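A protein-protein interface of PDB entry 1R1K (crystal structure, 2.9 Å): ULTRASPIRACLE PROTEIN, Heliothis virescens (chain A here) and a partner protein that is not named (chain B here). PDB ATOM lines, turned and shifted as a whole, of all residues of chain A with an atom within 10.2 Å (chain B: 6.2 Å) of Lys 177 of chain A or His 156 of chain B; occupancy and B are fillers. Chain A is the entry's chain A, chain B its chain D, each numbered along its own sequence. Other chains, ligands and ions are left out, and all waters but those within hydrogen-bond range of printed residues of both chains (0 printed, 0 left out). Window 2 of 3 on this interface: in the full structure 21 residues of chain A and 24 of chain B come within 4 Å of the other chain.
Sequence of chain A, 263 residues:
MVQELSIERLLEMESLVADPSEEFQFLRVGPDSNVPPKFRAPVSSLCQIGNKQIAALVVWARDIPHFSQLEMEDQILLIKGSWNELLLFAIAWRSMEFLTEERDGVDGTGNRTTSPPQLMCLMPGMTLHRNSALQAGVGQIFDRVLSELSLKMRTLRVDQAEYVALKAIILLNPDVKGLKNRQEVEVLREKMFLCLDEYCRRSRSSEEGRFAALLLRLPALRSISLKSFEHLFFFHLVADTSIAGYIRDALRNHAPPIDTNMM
The side-chain amino group (NZ) of Lys 177 of chain A lies within salt-bridge range of the side-chain carboxylate (OD1) of Asp 153 of chain B (3.4 Å). SG of Cys 160 of chain B sits at hydrogen-bond distance from OD1 of Asp 175 of chain A (3.2 Å). The guanidinium group of Arg 182 of chain A sits close to the side-chain sulfur of Cys 160 of chain B. NE2 of His 156 of chain B is in hydrogen-bond range of O of Asp 175 of chain A, at 2.6 Å. The side-chain carboxylate (OE2) of Glu 230 of chain B lies within salt-bridge range of the guanidinium group (NH2) of Arg 222 of chain A.
Of chain A, only Asp 175 and Lys 177 come within 4 Å of His 156 of chain B. No residue of chain A comes within 4 Å of Leu 155 of chain B. Cys 158 of chain B touches none of the printed residues of chain A. No residue of chain A comes within 4 Å of Arg 159 of chain B. Cys 160 of chain B touches just these residues of chain A: Asp 175 (3.2 Å) and Arg 182 (3.6 Å). Of the printed residues of chain A, Glu 230 of chain B touches Asp 175 (3.7 Å) and Arg 222 (3.1 Å). Printed residues of chain B within 4 Å of Arg 182 of chain A: Cys 160 (3.6 Å). Of the printed residues of chain B, Asp 175 of chain A touches His 156, Cys 160 and Glu 230. Lys 80 of chain A touches none of the printed residues of chain B. The nearest printed residue of chain A that does not touch Glu 230 of chain B is Asn 173 of chain A (4.1 Å).
The backbone NH (N) of Asp 175 of chain A lies within hydrogen-bond range of the side-chain amide oxygen (OD1) of Asn 173 of chain A, 3.2 Å away. The side-chain carboxylate (OE1) of Glu 186 of chain A is in salt-bridge range of the guanidinium group (NE) of Arg 182 of chain A, at 3.4 Å. NH2 of Arg 182 of chain A is in salt-bridge range of OD1 of Asp 175 of chain A, at 3.2 Å. O of His 156 of chain B is in hydrogen-bond range of SG of Cys 160 of chain B, at 3.5 Å.
Printed residues of chain A that touch a printed residue of chain B: Asp 175, Lys 177, Arg 182 and Arg 222. Hydrophobic or aromatic side chains of chain B that line the printed part of chain A: His 156. Among the printed residues, 7 pairs touch across the chains.
Glu 230 of chain B touches Asp 175 of chain A. Lys 177 of chain A touches His 156 of chain B.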
ATOM      1  N   GLU A  73      23.291  39.808 -28.428  1.00  0.00           N
ATOM      2  CA  GLU A  73      24.516  39.175 -28.933  1.00  0.00           C
ATOM      3  C   GLU A  73      24.344  37.656 -28.827  1.00  0.00           C
ATOM      4  O   GLU A  73      24.577  36.932 -29.790  1.00  0.00           O
ATOM      5  CB  GLU A  73      25.729  39.549 -28.091  1.00  0.00           C
ATOM      6  CG  GLU A  73      26.031  41.020 -27.937  1.00  0.00           C
ATOM      7  CD  GLU A  73      27.170  41.248 -26.933  1.00  0.00           C
ATOM      8  OE1 GLU A  73      28.269  40.683 -27.150  1.00  0.00           O
ATOM      9  OE2 GLU A  73      26.968  41.979 -25.929  1.00  0.00           O
ATOM     10  N   ASP A  74      23.948  37.189 -27.638  1.00  0.00           N
ATOM     11  CA  ASP A  74      23.714  35.762 -27.376  1.00  0.00           C
ATOM     12  C   ASP A  74      22.620  35.294 -28.310  1.00  0.00           C
ATOM     13  O   ASP A  74      22.807  34.356 -29.073  1.00  0.00           O
ATOM     14  CB  ASP A  74      23.241  35.523 -25.926  1.00  0.00           C
ATOM     15  CG  ASP A  74      24.393  35.432 -24.925  1.00  0.00           C
ATOM     16  OD1 ASP A  74      25.536  35.792 -25.289  1.00  0.00           O
ATOM     17  OD2 ASP A  74      24.143  35.003 -23.773  1.00  0.00           O
ATOM     18  N   GLN A  75      21.475  35.959 -28.226  1.00  0.00           N
ATOM     19  CA  GLN A  75      20.317  35.653 -29.060  1.00  0.00           C
ATOM     20  C   GLN A  75      20.731  35.328 -30.489  1.00  0.00           C
ATOM     21  O   GLN A  75      20.270  34.350 -31.073  1.00  0.00           O
ATOM     22  CB  GLN A  75      19.367  36.845 -29.068  1.00  0.00           C
ATOM     23  CG  GLN A  75      18.022  36.570 -28.454  1.00  0.00           C
ATOM     24  CD  GLN A  75      17.309  37.844 -28.075  1.00  0.00           C
ATOM     25  OE1 GLN A  75      17.239  38.787 -28.859  1.00  0.00           O
ATOM     26  NE2 GLN A  75      16.778  37.880 -26.867  1.00  0.00           N
ATOM     27  N   ILE A  76      21.597  36.164 -31.048  1.00  0.00           N
ATOM     28  CA  ILE A  76      22.090  35.952 -32.405  1.00  0.00           C
ATOM     29  C   ILE A  76      22.785  34.589 -32.443  1.00  0.00           C
ATOM     30  O   ILE A  76      22.390  33.679 -33.179  1.00  0.00           O
ATOM     31  CB  ILE A  76      23.117  37.050 -32.803  1.00  0.00           C
ATOM     32  CG1 ILE A  76      22.428  38.403 -32.918  1.00  0.00           C
ATOM     33  CG2 ILE A  76      23.779  36.699 -34.115  1.00  0.00           C
ATOM     34  CD1 ILE A  76      23.390  39.524 -33.074  1.00  0.00           C
ATOM     35  N   LEU A  77      23.819  34.466 -31.625  1.00  0.00           N
ATOM     36  CA  LEU A  77      24.594  33.252 -31.537  1.00  0.00           C
ATOM     37  C   LEU A  77      23.794  31.961 -31.335  1.00  0.00           C
ATOM     38  O   LEU A  77      24.169  30.908 -31.845  1.00  0.00           O
ATOM     39  CB  LEU A  77      25.641  33.414 -30.437  1.00  0.00           C
ATOM     40  CG  LEU A  77      27.025  33.878 -30.919  1.00  0.00           C
ATOM     41  CD1 LEU A  77      26.967  35.248 -31.552  1.00  0.00           C
ATOM     42  CD2 LEU A  77      27.963  33.886 -29.736  1.00  0.00           C
ATOM     43  N   LEU A  78      22.698  32.032 -30.596  1.00  0.00           N
ATOM     44  CA  LEU A  78      21.890  30.849 -30.354  1.00  0.00           C
ATOM     45  C   LEU A  78      21.209  30.412 -31.619  1.00  0.00           C
ATOM     46  O   LEU A  78      21.132  29.219 -31.915  1.00  0.00           O
ATOM     47  CB  LEU A  78      20.839  31.126 -29.286  1.00  0.00           C
ATOM     48  CG  LEU A  78      21.338  31.040 -27.845  1.00  0.00           C
ATOM     49  CD1 LEU A  78      20.171  31.237 -26.902  1.00  0.00           C
ATOM     50  CD2 LEU A  78      21.997  29.675 -27.605  1.00  0.00           C
ATOM     51  N   ILE A  79      20.697  31.393 -32.353  1.00  0.00           N
ATOM     52  CA  ILE A  79      20.019  31.146 -33.625  1.00  0.00           C
ATOM     53  C   ILE A  79      21.066  30.755 -34.668  1.00  0.00           C
ATOM     54  O   ILE A  79      20.997  29.682 -35.275  1.00  0.00           O
ATOM     55  CB  ILE A  79      19.251  32.400 -34.110  1.00  0.00           C
ATOM     56  CG1 ILE A  79      18.071  32.677 -33.181  1.00  0.00           C
ATOM     57  CG2 ILE A  79      18.749  32.184 -35.519  1.00  0.00           C
ATOM     58  CD1 ILE A  79      17.233  33.889 -33.571  1.00  0.00           C
ATOM     59  N   LYS A  80      22.036  31.640 -34.861  1.00  0.00           N
ATOM     60  CA  LYS A  80      23.113  31.414 -35.795  1.00  0.00           C
ATOM     61  C   LYS A  80      23.622  29.983 -35.607  1.00  0.00           C
ATOM     62  O   LYS A  80      24.060  29.354 -36.547  1.00  0.00           O
ATOM     63  CB  LYS A  80      24.238  32.420 -35.513  1.00  0.00           C
ATOM     64  CG  LYS A  80      25.295  32.551 -36.608  1.00  0.00           C
ATOM     65  CD  LYS A  80      26.675  32.878 -36.004  1.00  0.00           C
ATOM     66  CE  LYS A  80      27.798  33.045 -37.071  1.00  0.00           C
ATOM     67  NZ  LYS A  80      28.126  31.849 -37.940  1.00  0.00           N
ATOM     68  N   GLY A  81      23.538  29.459 -34.388  1.00  0.00           N
ATOM     69  CA  GLY A  81      24.039  28.128 -34.127  1.00  0.00           C
ATOM     70  C   GLY A  81      23.079  26.975 -34.295  1.00  0.00           C
ATOM     71  O   GLY A  81      23.504  25.829 -34.265  1.00  0.00           O
ATOM     72  N   SER A  82      21.793  27.246 -34.497  1.00  0.00           N
ATOM     73  CA  SER A  82      20.829  26.159 -34.641  1.00  0.00           C
ATOM     74  C   SER A  82      19.936  26.110 -35.909  1.00  0.00           C
ATOM     75  O   SER A  82      19.289  25.073 -36.166  1.00  0.00           O
ATOM     76  CB  SER A  82      19.951  26.131 -33.397  1.00  0.00           C
ATOM     77  OG  SER A  82      19.345  27.390 -33.186  1.00  0.00           O
ATOM     78  N   LEU A 171      17.228  24.843 -30.234  1.00  0.00           N
ATOM     79  CA  LEU A 171      17.600  26.249 -30.207  1.00  0.00           C
ATOM     80  C   LEU A 171      18.218  26.664 -28.877  1.00  0.00           C
ATOM     81  O   LEU A 171      19.237  27.354 -28.853  1.00  0.00           O
ATOM     82  CB  LEU A 171      16.380  27.145 -30.427  1.00  0.00           C
ATOM     83  CG  LEU A 171      16.611  28.633 -30.084  1.00  0.00           C
ATOM     84  CD1 LEU A 171      17.000  29.405 -31.332  1.00  0.00           C
ATOM     85  CD2 LEU A 171      15.344  29.223 -29.457  1.00  0.00           C
ATOM     86  N   ASN A 173      20.339  26.059 -26.579  1.00  0.00           N
ATOM     87  CA  ASN A 173      21.586  25.373 -26.241  1.00  0.00           C
ATOM     88  C   ASN A 173      22.599  26.300 -25.573  1.00  0.00           C
ATOM     89  O   ASN A 173      23.003  27.308 -26.140  1.00  0.00           O
ATOM     90  CB  ASN A 173      22.195  24.744 -27.503  1.00  0.00           C
ATOM     91  CG  ASN A 173      23.564  24.151 -27.266  1.00  0.00           C
ATOM     92  OD1 ASN A 173      23.768  23.347 -26.372  1.00  0.00           O
ATOM     93  ND2 ASN A 173      24.507  24.545 -28.081  1.00  0.00           N
ATOM     94  N   PRO A 174      23.016  25.954 -24.345  1.00  0.00           N
ATOM     95  CA  PRO A 174      23.975  26.680 -23.512  1.00  0.00           C
ATOM     96  C   PRO A 174      25.414  26.417 -23.933  1.00  0.00           C
ATOM     97  O   PRO A 174      26.302  27.206 -23.643  1.00  0.00           O
ATOM     98  CB  PRO A 174      23.727  26.111 -22.117  1.00  0.00           C
ATOM     99  CG  PRO A 174      22.454  25.316 -22.245  1.00  0.00           C
ATOM    100  CD  PRO A 174      22.498  24.789 -23.616  1.00  0.00           C
ATOM    101  N   ASP A 175      25.652  25.289 -24.589  1.00  0.00           N
ATOM    102  CA  ASP A 175      27.001  24.940 -25.014  1.00  0.00           C
ATOM    103  C   ASP A 175      27.534  25.769 -26.192  1.00  0.00           C
ATOM    104  O   ASP A 175      28.730  25.793 -26.456  1.00  0.00           O
ATOM    105  CB  ASP A 175      27.073  23.438 -25.298  1.00  0.00           C
ATOM    106  CG  ASP A 175      26.916  22.603 -24.027  1.00  0.00           C
ATOM    107  OD1 ASP A 175      27.578  22.955 -23.019  1.00  0.00           O
ATOM    108  OD2 ASP A 175      26.143  21.610 -24.034  1.00  0.00           O
ATOM    109  N   VAL A 176      26.650  26.464 -26.885  1.00  0.00           N
ATOM    110  CA  VAL A 176      27.070  27.326 -27.970  1.00  0.00           C
ATOM    111  C   VAL A 176      28.194  28.263 -27.497  1.00  0.00           C
ATOM    112  O   VAL A 176      28.005  29.040 -26.570  1.00  0.00           O
ATOM    113  CB  VAL A 176      25.885  28.139 -28.437  1.00  0.00           C
ATOM    114  CG1 VAL A 176      26.344  29.377 -29.196  1.00  0.00           C
ATOM    115  CG2 VAL A 176      25.004  27.253 -29.287  1.00  0.00           C
ATOM    116  N   LYS A 177      29.356  28.201 -28.142  1.00  0.00           N
ATOM    117  CA  LYS A 177      30.488  29.036 -27.743  1.00  0.00           C
ATOM    118  C   LYS A 177      30.241  30.557 -27.802  1.00  0.00           C
ATOM    119  O   LYS A 177      29.536  31.047 -28.675  1.00  0.00           O
ATOM    120  CB  LYS A 177      31.729  28.665 -28.566  1.00  0.00           C
ATOM    121  CG  LYS A 177      32.991  29.392 -28.128  1.00  0.00           C
ATOM    122  CD  LYS A 177      34.284  28.578 -28.341  1.00  0.00           C
ATOM    123  CE  LYS A 177      34.740  28.524 -29.803  1.00  0.00           C
ATOM    124  NZ  LYS A 177      33.692  27.990 -30.722  1.00  0.00           N
ATOM    125  N   GLY A 178      30.803  31.289 -26.841  1.00  0.00           N
ATOM    126  CA  GLY A 178      30.661  32.738 -26.800  1.00  0.00           C
ATOM    127  C   GLY A 178      29.467  33.335 -26.064  1.00  0.00           C
ATOM    128  O   GLY A 178      29.268  34.554 -26.092  1.00  0.00           O
ATOM    129  N   LEU A 179      28.661  32.513 -25.403  1.00  0.00           N
ATOM    130  CA  LEU A 179      27.502  33.053 -24.698  1.00  0.00           C
ATOM    131  C   LEU A 179      27.850  33.969 -23.524  1.00  0.00           C
ATOM    132  O   LEU A 179      28.360  33.520 -22.489  1.00  0.00           O
ATOM    133  CB  LEU A 179      26.591  31.923 -24.207  1.00  0.00           C
ATOM    134  CG  LEU A 179      25.779  31.189 -25.274  1.00  0.00           C
ATOM    135  CD1 LEU A 179      24.969  30.051 -24.623  1.00  0.00           C
ATOM    136  CD2 LEU A 179      24.880  32.184 -26.004  1.00  0.00           C
ATOM    137  N   LYS A 180      27.558  35.256 -23.695  1.00  0.00           N
ATOM    138  CA  LYS A 180      27.802  36.264 -22.660  1.00  0.00           C
ATOM    139  C   LYS A 180      27.394  35.718 -21.277  1.00  0.00           C
ATOM    140  O   LYS A 180      28.077  35.968 -20.284  1.00  0.00           O
ATOM    141  CB  LYS A 180      26.997  37.537 -22.986  1.00  0.00           C
ATOM    142  CG  LYS A 180      27.633  38.862 -22.577  1.00  0.00           C
ATOM    143  CD  LYS A 180      27.370  39.244 -21.114  1.00  0.00           C
ATOM    144  CE  LYS A 180      27.883  40.668 -20.790  1.00  0.00           C
ATOM    145  NZ  LYS A 180      27.170  41.744 -21.557  1.00  0.00           N
ATOM    146  N   ASN A 181      26.287  34.971 -21.218  1.00  0.00           N
ATOM    147  CA  ASN A 181      25.808  34.393 -19.957  1.00  0.00           C
ATOM    148  C   ASN A 181      25.140  33.040 -20.115  1.00  0.00           C
ATOM    149  O   ASN A 181      23.917  32.933 -20.112  1.00  0.00           O
ATOM    150  CB  ASN A 181      24.847  35.350 -19.276  1.00  0.00           C
ATOM    151  CG  ASN A 181      24.182  36.260 -20.249  1.00  0.00           C
ATOM    152  OD1 ASN A 181      23.343  35.832 -21.051  1.00  0.00           O
ATOM    153  ND2 ASN A 181      24.567  37.535 -20.213  1.00  0.00           N
ATOM    154  N   ARG A 182      25.976  32.011 -20.220  1.00  0.00           N
ATOM    155  CA  ARG A 182      25.547  30.628 -20.390  1.00  0.00           C
ATOM    156  C   ARG A 182      24.384  30.176 -19.509  1.00  0.00           C
ATOM    157  O   ARG A 182      23.428  29.574 -19.985  1.00  0.00           O
ATOM    158  CB  ARG A 182      26.736  29.698 -20.154  1.00  0.00           C
ATOM    159  CG  ARG A 182      26.438  28.235 -20.413  1.00  0.00           C
ATOM    160  CD  ARG A 182      27.526  27.325 -19.861  1.00  0.00           C
ATOM    161  NE  ARG A 182      27.270  25.925 -20.191  1.00  0.00           N
ATOM    162  CZ  ARG A 182      27.703  24.897 -19.466  1.00  0.00           C
ATOM    163  NH1 ARG A 182      28.411  25.109 -18.361  1.00  0.00           N
ATOM    164  NH2 ARG A 182      27.441  23.649 -19.851  1.00  0.00           N
ATOM    165  N   VAL A 185      20.782  30.748 -20.279  1.00  0.00           N
ATOM    166  CA  VAL A 185      20.198  29.856 -21.274  1.00  0.00           C
ATOM    167  C   VAL A 185      19.898  28.506 -20.607  1.00  0.00           C
ATOM    168  O   VAL A 185      18.841  27.915 -20.848  1.00  0.00           O
ATOM    169  CB  VAL A 185      21.147  29.641 -22.467  1.00  0.00           C
ATOM    170  CG1 VAL A 185      20.465  28.804 -23.522  1.00  0.00           C
ATOM    171  CG2 VAL A 185      21.566  30.972 -23.036  1.00  0.00           C
ATOM    172  N   GLU A 186      20.823  28.040 -19.761  1.00  0.00           N
ATOM    173  CA  GLU A 186      20.663  26.770 -19.043  1.00  0.00           C
ATOM    174  C   GLU A 186      19.293  26.680 -18.345  1.00  0.00           C
ATOM    175  O   GLU A 186      18.701  25.598 -18.243  1.00  0.00           O
ATOM    176  CB  GLU A 186      21.748  26.597 -17.975  1.00  0.00           C
ATOM    177  CG  GLU A 186      23.184  26.487 -18.439  1.00  0.00           C
ATOM    178  CD  GLU A 186      24.149  26.371 -17.245  1.00  0.00           C
ATOM    179  OE1 GLU A 186      25.389  26.345 -17.445  1.00  0.00           O
ATOM    180  OE2 GLU A 186      23.657  26.308 -16.092  1.00  0.00           O
ATOM    181  N   ARG A 222      22.542  16.561 -35.185  1.00  0.00           N
ATOM    182  CA  ARG A 222      23.729  17.398 -35.186  1.00  0.00           C
ATOM    183  C   ARG A 222      24.701  16.938 -36.267  1.00  0.00           C
ATOM    184  O   ARG A 222      25.281  17.751 -37.000  1.00  0.00           O
ATOM    185  CB  ARG A 222      24.385  17.341 -33.799  1.00  0.00           C
ATOM    186  CG  ARG A 222      25.841  17.809 -33.744  1.00  0.00           C
ATOM    187  CD  ARG A 222      25.983  19.241 -34.148  1.00  0.00           C
ATOM    188  NE  ARG A 222      25.191  20.058 -33.249  1.00  0.00           N
ATOM    189  CZ  ARG A 222      25.561  20.364 -32.014  1.00  0.00           C
ATOM    190  NH1 ARG A 222      26.724  19.925 -31.541  1.00  0.00           N
ATOM    191  NH2 ARG A 222      24.767  21.089 -31.245  1.00  0.00           N
ATOM    192  N   ILE B 151      41.890  22.834 -30.794  1.00  0.00           N
ATOM    193  CA  ILE B 151      41.924  23.222 -29.397  1.00  0.00           C
ATOM    194  C   ILE B 151      40.933  24.201 -28.780  1.00  0.00           C
ATOM    195  O   ILE B 151      40.422  23.913 -27.695  1.00  0.00           O
ATOM    196  CB  ILE B 151      43.379  23.614 -28.981  1.00  0.00           C
ATOM    197  CG1 ILE B 151      43.587  23.326 -27.493  1.00  0.00           C
ATOM    198  CG2 ILE B 151      43.649  25.064 -29.283  1.00  0.00           C
ATOM    199  CD1 ILE B 151      43.209  21.909 -27.087  1.00  0.00           C
ATOM    200  N   GLU B 152      40.632  25.330 -29.419  1.00  0.00           N
ATOM    201  CA  GLU B 152      39.688  26.276 -28.798  1.00  0.00           C
ATOM    202  C   GLU B 152      38.322  25.689 -28.469  1.00  0.00           C
ATOM    203  O   GLU B 152      37.711  26.060 -27.461  1.00  0.00           O
ATOM    204  CB  GLU B 152      39.491  27.550 -29.647  1.00  0.00           C
ATOM    205  CG  GLU B 152      40.378  28.751 -29.224  1.00  0.00           C
ATOM    206  CD  GLU B 152      40.780  28.717 -27.728  1.00  0.00           C
ATOM    207  OE1 GLU B 152      39.878  28.694 -26.838  1.00  0.00           O
ATOM    208  OE2 GLU B 152      42.007  28.715 -27.445  1.00  0.00           O
ATOM    209  N   ASP B 153      37.856  24.767 -29.310  1.00  0.00           N
ATOM    210  CA  ASP B 153      36.558  24.108 -29.134  1.00  0.00           C
ATOM    211  C   ASP B 153      36.663  22.948 -28.145  1.00  0.00           C
ATOM    212  O   ASP B 153      35.754  22.707 -27.366  1.00  0.00           O
ATOM    213  CB  ASP B 153      36.045  23.574 -30.494  1.00  0.00           C
ATOM    214  CG  ASP B 153      34.761  24.260 -30.962  1.00  0.00           C
ATOM    215  OD1 ASP B 153      34.795  25.025 -31.950  1.00  0.00           O
ATOM    216  OD2 ASP B 153      33.706  24.031 -30.334  1.00  0.00           O
ATOM    217  N   LEU B 154      37.779  22.229 -28.192  1.00  0.00           N
ATOM    218  CA  LEU B 154      37.992  21.070 -27.320  1.00  0.00           C
ATOM    219  C   LEU B 154      38.062  21.494 -25.858  1.00  0.00           C
ATOM    220  O   LEU B 154      37.569  20.798 -24.951  1.00  0.00           O
ATOM    221  CB  LEU B 154      39.288  20.361 -27.691  1.00  0.00           C
ATOM    222  CG  LEU B 154      39.371  18.976 -27.069  1.00  0.00           C
ATOM    223  CD1 LEU B 154      38.625  17.994 -27.938  1.00  0.00           C
ATOM    224  CD2 LEU B 154      40.792  18.555 -26.930  1.00  0.00           C
ATOM    225  N   LEU B 155      38.690  22.646 -25.654  1.00  0.00           N
ATOM    226  CA  LEU B 155      38.855  23.226 -24.338  1.00  0.00           C
ATOM    227  C   LEU B 155      37.513  23.842 -23.823  1.00  0.00           C
ATOM    228  O   LEU B 155      37.263  23.869 -22.631  1.00  0.00           O
ATOM    229  CB  LEU B 155      39.972  24.271 -24.418  1.00  0.00           C
ATOM    230  CG  LEU B 155      41.245  24.218 -23.574  1.00  0.00           C
ATOM    231  CD1 LEU B 155      41.881  22.834 -23.580  1.00  0.00           C
ATOM    232  CD2 LEU B 155      42.191  25.264 -24.119  1.00  0.00           C
ATOM    233  N   HIS B 156      36.658  24.335 -24.720  1.00  0.00           N
ATOM    234  CA  HIS B 156      35.357  24.907 -24.340  1.00  0.00           C
ATOM    235  C   HIS B 156      34.470  23.754 -23.833  1.00  0.00           C
ATOM    236  O   HIS B 156      33.723  23.870 -22.867  1.00  0.00           O
ATOM    237  CB  HIS B 156      34.716  25.548 -25.576  1.00  0.00           C
ATOM    238  CG  HIS B 156      33.270  25.913 -25.406  1.00  0.00           C
ATOM    239  ND1 HIS B 156      32.856  27.174 -25.020  1.00  0.00           N
ATOM    240  CD2 HIS B 156      32.139  25.178 -25.555  1.00  0.00           C
ATOM    241  CE1 HIS B 156      31.537  27.195 -24.936  1.00  0.00           C
ATOM    242  NE2 HIS B 156      31.077  25.999 -25.253  1.00  0.00           N
ATOM    243  N   PHE B 157      34.559  22.629 -24.519  1.00  0.00           N
ATOM    244  CA  PHE B 157      33.789  21.475 -24.144  1.00  0.00           C
ATOM    245  C   PHE B 157      34.203  21.029 -22.758  1.00  0.00           C
ATOM    246  O   PHE B 157      33.374  20.538 -22.015  1.00  0.00           O
ATOM    247  CB  PHE B 157      34.021  20.353 -25.163  1.00  0.00           C
ATOM    248  CG  PHE B 157      33.411  19.035 -24.767  1.00  0.00           C
ATOM    249  CD1 PHE B 157      32.068  18.802 -24.930  1.00  0.00           C
ATOM    250  CD2 PHE B 157      34.201  18.022 -24.243  1.00  0.00           C
ATOM    251  CE1 PHE B 157      31.515  17.567 -24.577  1.00  0.00           C
ATOM    252  CE2 PHE B 157      33.660  16.790 -23.888  1.00  0.00           C
ATOM    253  CZ  PHE B 157      32.319  16.560 -24.054  1.00  0.00           C
ATOM    254  N   CYS B 158      35.491  21.176 -22.433  1.00  0.00           N
ATOM    255  CA  CYS B 158      36.038  20.793 -21.128  1.00  0.00           C
ATOM    256  C   CYS B 158      35.507  21.707 -20.033  1.00  0.00           C
ATOM    257  O   CYS B 158      35.083  21.252 -18.980  1.00  0.00           O
ATOM    258  CB  CYS B 158      37.558  20.850 -21.149  1.00  0.00           C
ATOM    259  SG  CYS B 158      38.290  19.513 -22.132  1.00  0.00           S
ATOM    260  N   ARG B 159      35.526  23.005 -20.272  1.00  0.00           N
ATOM    261  CA  ARG B 159      34.975  23.915 -19.308  1.00  0.00           C
ATOM    262  C   ARG B 159      33.504  23.532 -19.078  1.00  0.00           C
ATOM    263  O   ARG B 159      33.050  23.500 -17.944  1.00  0.00           O
ATOM    264  CB  ARG B 159      35.148  25.343 -19.801  1.00  0.00           C
ATOM    265  CG  ARG B 159      36.624  25.755 -19.848  1.00  0.00           C
ATOM    266  CD  ARG B 159      36.839  27.197 -20.289  1.00  0.00           C
ATOM    267  NE  ARG B 159      36.743  27.407 -21.741  1.00  0.00           N
ATOM    268  CZ  ARG B 159      37.768  27.356 -22.593  1.00  0.00           C
ATOM    269  NH1 ARG B 159      38.999  27.103 -22.159  1.00  0.00           N
ATOM    270  NH2 ARG B 159      37.558  27.555 -23.889  1.00  0.00           N
ATOM    271  N   CYS B 160      32.763  23.196 -20.125  1.00  0.00           N
ATOM    272  CA  CYS B 160      31.361  22.801 -19.949  1.00  0.00           C
ATOM    273  C   CYS B 160      31.150  21.457 -19.246  1.00  0.00           C
ATOM    274  O   CYS B 160      30.087  21.209 -18.682  1.00  0.00           O
ATOM    275  CB  CYS B 160      30.638  22.710 -21.282  1.00  0.00           C
ATOM    276  SG  CYS B 160      30.337  24.246 -22.089  1.00  0.00           S
ATOM    277  N   MET B 161      32.134  20.570 -19.316  1.00  0.00           N
ATOM    278  CA  MET B 161      32.025  19.261 -18.688  1.00  0.00           C
ATOM    279  C   MET B 161      32.450  19.380 -17.240  1.00  0.00           C
ATOM    280  O   MET B 161      32.088  18.575 -16.381  1.00  0.00           O
ATOM    281  CB  MET B 161      32.927  18.281 -19.416  1.00  0.00           C
ATOM    282  CG  MET B 161      32.450  17.987 -20.787  1.00  0.00           C
ATOM    283  SD  MET B 161      30.994  16.963 -20.704  1.00  0.00           S
ATOM    284  CE  MET B 161      31.739  15.248 -20.744  1.00  0.00           C
ATOM    285  N   GLU B 230      27.076  17.216 -28.475  1.00  0.00           N
ATOM    286  CA  GLU B 230      28.281  18.038 -28.577  1.00  0.00           C
ATOM    287  C   GLU B 230      29.489  17.193 -29.041  1.00  0.00           C
ATOM    288  O   GLU B 230      30.362  17.632 -29.810  1.00  0.00           O
ATOM    289  CB  GLU B 230      28.562  18.685 -27.222  1.00  0.00           C
ATOM    290  CG  GLU B 230      27.521  19.686 -26.903  1.00  0.00           C
ATOM    291  CD  GLU B 230      27.411  20.685 -28.014  1.00  0.00           C
ATOM    292  OE1 GLU B 230      28.466  21.240 -28.369  1.00  0.00           O
ATOM    293  OE2 GLU B 230      26.299  20.912 -28.541  1.00  0.00           O
